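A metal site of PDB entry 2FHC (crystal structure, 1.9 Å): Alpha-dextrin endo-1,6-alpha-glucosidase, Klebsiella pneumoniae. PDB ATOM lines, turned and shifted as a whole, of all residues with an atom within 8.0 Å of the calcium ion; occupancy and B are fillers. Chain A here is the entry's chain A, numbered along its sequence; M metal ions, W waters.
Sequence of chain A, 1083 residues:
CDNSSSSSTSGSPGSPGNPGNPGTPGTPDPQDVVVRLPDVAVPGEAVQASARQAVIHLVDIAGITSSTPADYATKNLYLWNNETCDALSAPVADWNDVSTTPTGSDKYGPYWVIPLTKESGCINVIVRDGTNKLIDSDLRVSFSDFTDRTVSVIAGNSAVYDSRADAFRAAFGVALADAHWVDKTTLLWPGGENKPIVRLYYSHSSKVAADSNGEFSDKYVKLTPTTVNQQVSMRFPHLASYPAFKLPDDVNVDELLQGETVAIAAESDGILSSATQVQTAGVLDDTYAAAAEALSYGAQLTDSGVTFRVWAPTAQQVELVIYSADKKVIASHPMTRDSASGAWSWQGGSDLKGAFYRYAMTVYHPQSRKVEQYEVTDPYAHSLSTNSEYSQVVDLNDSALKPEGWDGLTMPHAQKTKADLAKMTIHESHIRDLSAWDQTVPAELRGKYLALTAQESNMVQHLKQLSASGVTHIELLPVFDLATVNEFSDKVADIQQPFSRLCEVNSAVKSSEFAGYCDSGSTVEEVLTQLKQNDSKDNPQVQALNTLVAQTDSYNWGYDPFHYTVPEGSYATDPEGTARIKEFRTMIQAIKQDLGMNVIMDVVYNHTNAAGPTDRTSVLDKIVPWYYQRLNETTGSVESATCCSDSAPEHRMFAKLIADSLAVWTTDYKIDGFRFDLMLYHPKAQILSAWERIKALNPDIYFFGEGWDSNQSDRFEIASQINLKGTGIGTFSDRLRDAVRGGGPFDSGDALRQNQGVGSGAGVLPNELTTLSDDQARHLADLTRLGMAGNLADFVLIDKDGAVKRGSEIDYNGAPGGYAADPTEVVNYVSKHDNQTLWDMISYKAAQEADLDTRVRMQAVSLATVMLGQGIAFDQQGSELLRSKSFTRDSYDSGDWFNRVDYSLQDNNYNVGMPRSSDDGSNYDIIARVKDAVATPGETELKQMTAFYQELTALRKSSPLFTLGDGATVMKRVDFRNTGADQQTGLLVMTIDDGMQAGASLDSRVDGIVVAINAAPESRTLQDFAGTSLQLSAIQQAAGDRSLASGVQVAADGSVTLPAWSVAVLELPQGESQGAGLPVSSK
Within 4 Å of the calcium ion: Ala 550, Asp 553, Tyr 555 and Asp 893.
The nearest printed residue that does not touch the calcium ion is Asn 556 (4.6 Å).
The calcium ion is bound by the backbone carbonyl oxygen of Tyr 555, the side-chain carboxylate of Asp 893, the backbone carbonyl oxygen of Ala 550, the side-chain carboxylate of Asp 553, water W1, water W3 and water W2.
Water W3 lies within hydrogen-bond range of the backbone carbonyl oxygen (O) of Thr 484 (2.9 Å) and the side-chain amide nitrogen (ND2) of Asn 556 (3.1 Å).
Water W1 bridges O of Asp 553 (2.7 Å) and O of Thr 484 (3.4 Å).
Water W2 lies within hydrogen-bond range of OD2 of Asp 553 (2.7 Å), O of Asp 893 (3.0 Å) and N of Gly 895 (3.2 Å).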
ATOM      1  N   THR A 484       2.286  21.832 -36.457  1.00  0.00           N
ATOM      2  CA  THR A 484       1.522  20.977 -35.560  1.00  0.00           C
ATOM      3  C   THR A 484       0.369  21.525 -34.704  1.00  0.00           C
ATOM      4  O   THR A 484      -0.057  20.875 -33.740  1.00  0.00           O
ATOM      5  CB  THR A 484       2.498  20.189 -34.684  1.00  0.00           C
ATOM      6  OG1 THR A 484       3.517  21.056 -34.186  1.00  0.00           O
ATOM      7  CG2 THR A 484       3.166  19.092 -35.523  1.00  0.00           C
ATOM      8  N   VAL A 485      -0.134  22.702 -35.071  1.00  0.00           N
ATOM      9  CA  VAL A 485      -1.289  23.311 -34.406  1.00  0.00           C
ATOM     10  C   VAL A 485      -2.194  23.857 -35.521  1.00  0.00           C
ATOM     11  O   VAL A 485      -1.744  24.633 -36.359  1.00  0.00           O
ATOM     12  CB  VAL A 485      -0.903  24.483 -33.477  1.00  0.00           C
ATOM     13  CG1 VAL A 485      -2.162  25.265 -33.060  1.00  0.00           C
ATOM     14  CG2 VAL A 485      -0.196  23.955 -32.223  1.00  0.00           C
ATOM     15  N   ASN A 486      -3.457  23.434 -35.545  1.00  0.00           N
ATOM     16  CA  ASN A 486      -4.367  23.907 -36.592  1.00  0.00           C
ATOM     17  C   ASN A 486      -4.753  25.355 -36.289  1.00  0.00           C
ATOM     18  O   ASN A 486      -5.229  25.667 -35.196  1.00  0.00           O
ATOM     19  CB  ASN A 486      -5.623  23.027 -36.639  1.00  0.00           C
ATOM     20  CG  ASN A 486      -6.399  23.195 -37.945  1.00  0.00           C
ATOM     21  OD1 ASN A 486      -6.692  24.314 -38.365  1.00  0.00           O
ATOM     22  ND2 ASN A 486      -6.731  22.083 -38.579  1.00  0.00           N
ATOM     23  N   ASP A 494      -9.699  23.277 -26.662  1.00  0.00           N
ATOM     24  CA  ASP A 494      -8.747  23.341 -25.553  1.00  0.00           C
ATOM     25  C   ASP A 494      -9.413  22.916 -24.238  1.00  0.00           C
ATOM     26  O   ASP A 494     -10.646  22.890 -24.137  1.00  0.00           O
ATOM     27  CB  ASP A 494      -8.155  24.748 -25.473  1.00  0.00           C
ATOM     28  CG  ASP A 494      -7.115  24.983 -26.568  1.00  0.00           C
ATOM     29  OD1 ASP A 494      -6.079  24.277 -26.555  1.00  0.00           O
ATOM     30  OD2 ASP A 494      -7.318  25.858 -27.443  1.00  0.00           O
ATOM     31  N   ASN A 546      -5.681  12.863 -21.784  1.00  0.00           N
ATOM     32  CA  ASN A 546      -4.869  13.956 -22.305  1.00  0.00           C
ATOM     33  C   ASN A 546      -4.199  13.607 -23.637  1.00  0.00           C
ATOM     34  O   ASN A 546      -4.024  14.472 -24.494  1.00  0.00           O
ATOM     35  CB  ASN A 546      -3.809  14.378 -21.286  1.00  0.00           C
ATOM     36  CG  ASN A 546      -3.282  15.784 -21.547  1.00  0.00           C
ATOM     37  OD1 ASN A 546      -4.068  16.732 -21.635  1.00  0.00           O
ATOM     38  ND2 ASN A 546      -1.971  15.925 -21.651  1.00  0.00           N
ATOM     39  N   THR A 547      -3.824  12.338 -23.804  1.00  0.00           N
ATOM     40  CA  THR A 547      -3.187  11.907 -25.037  1.00  0.00           C
ATOM     41  C   THR A 547      -4.109  12.155 -26.234  1.00  0.00           C
ATOM     42  O   THR A 547      -3.649  12.435 -27.342  1.00  0.00           O
ATOM     43  CB  THR A 547      -2.799  10.418 -24.970  1.00  0.00           C
ATOM     44  OG1 THR A 547      -1.741  10.260 -24.012  1.00  0.00           O
ATOM     45  CG2 THR A 547      -2.315   9.912 -26.338  1.00  0.00           C
ATOM     46  N   LEU A 548      -5.416  12.034 -26.004  1.00  0.00           N
ATOM     47  CA  LEU A 548      -6.381  12.269 -27.058  1.00  0.00           C
ATOM     48  C   LEU A 548      -6.565  13.775 -27.263  1.00  0.00           C
ATOM     49  O   LEU A 548      -6.605  14.253 -28.394  1.00  0.00           O
ATOM     50  CB  LEU A 548      -7.730  11.627 -26.698  1.00  0.00           C
ATOM     51  CG  LEU A 548      -7.655  10.108 -26.490  1.00  0.00           C
ATOM     52  CD1 LEU A 548      -9.021   9.551 -26.104  1.00  0.00           C
ATOM     53  CD2 LEU A 548      -7.159   9.441 -27.777  1.00  0.00           C
ATOM     54  N   VAL A 549      -6.650  14.508 -26.159  1.00  0.00           N
ATOM     55  CA  VAL A 549      -6.797  15.966 -26.210  1.00  0.00           C
ATOM     56  C   VAL A 549      -5.644  16.628 -26.986  1.00  0.00           C
ATOM     57  O   VAL A 549      -5.856  17.589 -27.741  1.00  0.00           O
ATOM     58  CB  VAL A 549      -6.822  16.566 -24.769  1.00  0.00           C
ATOM     59  CG1 VAL A 549      -6.753  18.097 -24.832  1.00  0.00           C
ATOM     60  CG2 VAL A 549      -8.104  16.131 -24.051  1.00  0.00           C
ATOM     61  N   ALA A 550      -4.444  16.093 -26.819  1.00  0.00           N
ATOM     62  CA  ALA A 550      -3.245  16.633 -27.472  1.00  0.00           C
ATOM     63  C   ALA A 550      -3.324  16.694 -29.001  1.00  0.00           C
ATOM     64  O   ALA A 550      -2.656  17.515 -29.630  1.00  0.00           O
ATOM     65  CB  ALA A 550      -2.032  15.822 -27.041  1.00  0.00           C
ATOM     66  N   GLN A 551      -4.148  15.831 -29.582  1.00  0.00           N
ATOM     67  CA  GLN A 551      -4.294  15.765 -31.042  1.00  0.00           C
ATOM     68  C   GLN A 551      -4.982  16.963 -31.670  1.00  0.00           C
ATOM     69  O   GLN A 551      -4.696  17.324 -32.811  1.00  0.00           O
ATOM     70  CB  GLN A 551      -5.085  14.500 -31.419  1.00  0.00           C
ATOM     71  CG  GLN A 551      -4.467  13.204 -30.941  1.00  0.00           C
ATOM     72  CD  GLN A 551      -5.414  12.030 -31.074  1.00  0.00           C
ATOM     73  OE1 GLN A 551      -5.002  10.874 -30.926  1.00  0.00           O
ATOM     74  NE2 GLN A 551      -6.678  12.310 -31.357  1.00  0.00           N
ATOM     75  N   THR A 552      -5.886  17.597 -30.925  1.00  0.00           N
ATOM     76  CA  THR A 552      -6.638  18.724 -31.452  1.00  0.00           C
ATOM     77  C   THR A 552      -6.643  19.995 -30.606  1.00  0.00           C
ATOM     78  O   THR A 552      -7.542  20.818 -30.754  1.00  0.00           O
ATOM     79  CB  THR A 552      -8.119  18.313 -31.713  1.00  0.00           C
ATOM     80  OG1 THR A 552      -8.646  17.638 -30.564  1.00  0.00           O
ATOM     81  CG2 THR A 552      -8.213  17.378 -32.901  1.00  0.00           C
ATOM     82  N   ASP A 553      -5.655  20.161 -29.735  1.00  0.00           N
ATOM     83  CA  ASP A 553      -5.589  21.373 -28.913  1.00  0.00           C
ATOM     84  C   ASP A 553      -4.673  22.423 -29.555  1.00  0.00           C
ATOM     85  O   ASP A 553      -4.204  22.231 -30.676  1.00  0.00           O
ATOM     86  CB  ASP A 553      -5.116  21.049 -27.478  1.00  0.00           C
ATOM     87  CG  ASP A 553      -3.717  20.430 -27.422  1.00  0.00           C
ATOM     88  OD1 ASP A 553      -3.005  20.412 -28.448  1.00  0.00           O
ATOM     89  OD2 ASP A 553      -3.337  19.962 -26.330  1.00  0.00           O
ATOM     90  N   SER A 554      -4.444  23.533 -28.856  1.00  0.00           N
ATOM     91  CA  SER A 554      -3.603  24.606 -29.389  1.00  0.00           C
ATOM     92  C   SER A 554      -2.148  24.467 -28.938  1.00  0.00           C
ATOM     93  O   SER A 554      -1.344  25.377 -29.165  1.00  0.00           O
ATOM     94  CB  SER A 554      -4.120  25.964 -28.901  1.00  0.00           C
ATOM     95  OG  SER A 554      -5.450  26.207 -29.316  1.00  0.00           O
ATOM     96  N   TYR A 555      -1.802  23.344 -28.320  1.00  0.00           N
ATOM     97  CA  TYR A 555      -0.471  23.162 -27.771  1.00  0.00           C
ATOM     98  C   TYR A 555       0.581  22.285 -28.462  1.00  0.00           C
ATOM     99  O   TYR A 555       0.305  21.138 -28.841  1.00  0.00           O
ATOM    100  CB  TYR A 555      -0.597  22.674 -26.316  1.00  0.00           C
ATOM    101  CG  TYR A 555       0.675  22.800 -25.513  1.00  0.00           C
ATOM    102  CD1 TYR A 555       1.765  21.956 -25.736  1.00  0.00           C
ATOM    103  CD2 TYR A 555       0.834  23.833 -24.585  1.00  0.00           C
ATOM    104  CE1 TYR A 555       2.986  22.143 -25.075  1.00  0.00           C
ATOM    105  CE2 TYR A 555       2.029  24.031 -23.915  1.00  0.00           C
ATOM    106  CZ  TYR A 555       3.104  23.182 -24.166  1.00  0.00           C
ATOM    107  OH  TYR A 555       4.305  23.418 -23.533  1.00  0.00           O
ATOM    108  N   ASN A 556       1.788  22.838 -28.590  1.00  0.00           N
ATOM    109  CA  ASN A 556       2.957  22.120 -29.106  1.00  0.00           C
ATOM    110  C   ASN A 556       4.166  23.034 -28.982  1.00  0.00           C
ATOM    111  O   ASN A 556       4.062  24.246 -29.139  1.00  0.00           O
ATOM    112  CB  ASN A 556       2.778  21.674 -30.561  1.00  0.00           C
ATOM    113  CG  ASN A 556       3.765  20.575 -30.959  1.00  0.00           C
ATOM    114  OD1 ASN A 556       4.958  20.814 -31.099  1.00  0.00           O
ATOM    115  ND2 ASN A 556       3.256  19.356 -31.112  1.00  0.00           N
ATOM    116  N   TRP A 557       5.329  22.454 -28.668  1.00  0.00           N
ATOM    117  CA  TRP A 557       6.547  23.256 -28.566  1.00  0.00           C
ATOM    118  C   TRP A 557       6.787  23.919 -29.918  1.00  0.00           C
ATOM    119  O   TRP A 557       7.290  25.053 -29.987  1.00  0.00           O
ATOM    120  CB  TRP A 557       7.762  22.390 -28.220  1.00  0.00           C
ATOM    121  CG  TRP A 557       7.857  21.988 -26.779  1.00  0.00           C
ATOM    122  CD1 TRP A 557       7.164  22.502 -25.720  1.00  0.00           C
ATOM    123  CD2 TRP A 557       8.728  20.986 -26.247  1.00  0.00           C
ATOM    124  NE1 TRP A 557       7.555  21.887 -24.556  1.00  0.00           N
ATOM    125  CE2 TRP A 557       8.510  20.948 -24.845  1.00  0.00           C
ATOM    126  CE3 TRP A 557       9.676  20.116 -26.808  1.00  0.00           C
ATOM    127  CZ2 TRP A 557       9.204  20.075 -24.009  1.00  0.00           C
ATOM    128  CZ3 TRP A 557      10.355  19.240 -25.976  1.00  0.00           C
ATOM    129  CH2 TRP A 557      10.120  19.222 -24.583  1.00  0.00           C
ATOM    130  N   TYR A 892       6.675  17.910 -25.157  1.00  0.00           N
ATOM    131  CA  TYR A 892       6.358  18.666 -26.367  1.00  0.00           C
ATOM    132  C   TYR A 892       4.899  18.707 -26.828  1.00  0.00           C
ATOM    133  O   TYR A 892       4.460  19.703 -27.396  1.00  0.00           O
ATOM    134  CB  TYR A 892       7.224  18.183 -27.539  1.00  0.00           C
ATOM    135  CG  TYR A 892       6.769  16.878 -28.147  1.00  0.00           C
ATOM    136  CD1 TYR A 892       6.937  15.666 -27.472  1.00  0.00           C
ATOM    137  CD2 TYR A 892       6.159  16.856 -29.404  1.00  0.00           C
ATOM    138  CE1 TYR A 892       6.497  14.467 -28.025  1.00  0.00           C
ATOM    139  CE2 TYR A 892       5.713  15.658 -29.966  1.00  0.00           C
ATOM    140  CZ  TYR A 892       5.895  14.467 -29.273  1.00  0.00           C
ATOM    141  OH  TYR A 892       5.475  13.289 -29.838  1.00  0.00           O
ATOM    142  N   ASP A 893       4.159  17.632 -26.586  1.00  0.00           N
ATOM    143  CA  ASP A 893       2.762  17.552 -26.999  1.00  0.00           C
ATOM    144  C   ASP A 893       1.868  17.170 -25.809  1.00  0.00           C
ATOM    145  O   ASP A 893       0.779  16.630 -25.993  1.00  0.00           O
ATOM    146  CB  ASP A 893       2.616  16.501 -28.102  1.00  0.00           C
ATOM    147  CG  ASP A 893       1.348  16.660 -28.916  1.00  0.00           C
ATOM    148  OD1 ASP A 893       0.985  15.687 -29.619  1.00  0.00           O
ATOM    149  OD2 ASP A 893       0.721  17.732 -28.879  1.00  0.00           O
ATOM    150  N   SER A 894       2.335  17.464 -24.593  1.00  0.00           N
ATOM    151  CA  SER A 894       1.575  17.128 -23.383  1.00  0.00           C
ATOM    152  C   SER A 894       0.579  18.197 -22.944  1.00  0.00           C
ATOM    153  O   SER A 894       0.072  18.162 -21.815  1.00  0.00           O
ATOM    154  CB  SER A 894       2.538  16.791 -22.241  1.00  0.00           C
ATOM    155  OG  SER A 894       3.221  15.572 -22.519  1.00  0.00           O
ATOM    156  N   GLY A 895       0.324  19.167 -23.816  1.00  0.00           N
ATOM    157  CA  GLY A 895      -0.649  20.214 -23.562  1.00  0.00           C
ATOM    158  C   GLY A 895      -0.529  21.134 -22.370  1.00  0.00           C
ATOM    159  O   GLY A 895       0.483  21.159 -21.664  1.00  0.00           O
ATOM    160  N   ASP A 896      -1.584  21.920 -22.143  1.00  0.00           N
ATOM    161  CA  ASP A 896      -1.643  22.863 -21.041  1.00  0.00           C
ATOM    162  C   ASP A 896      -1.578  22.177 -19.669  1.00  0.00           C
ATOM    163  O   ASP A 896      -1.034  22.744 -18.722  1.00  0.00           O
ATOM    164  CB  ASP A 896      -2.944  23.689 -21.090  1.00  0.00           C
ATOM    165  CG  ASP A 896      -3.023  24.626 -22.287  1.00  0.00           C
ATOM    166  OD1 ASP A 896      -1.962  25.043 -22.792  1.00  0.00           O
ATOM    167  OD2 ASP A 896      -4.161  24.960 -22.694  1.00  0.00           O
HETATM  168 CA    CA M   1      -1.047  19.273 -29.340  1.00  0.00          CA
HETATM  169  O   HOH W   1      -2.209  20.409 -31.156  1.00  0.00           O
HETATM  170  O   HOH W   2      -0.839  18.992 -26.783  1.00  0.00           O
HETATM  171  O   HOH W   3       0.231  18.998 -31.556  1.00  0.00           O
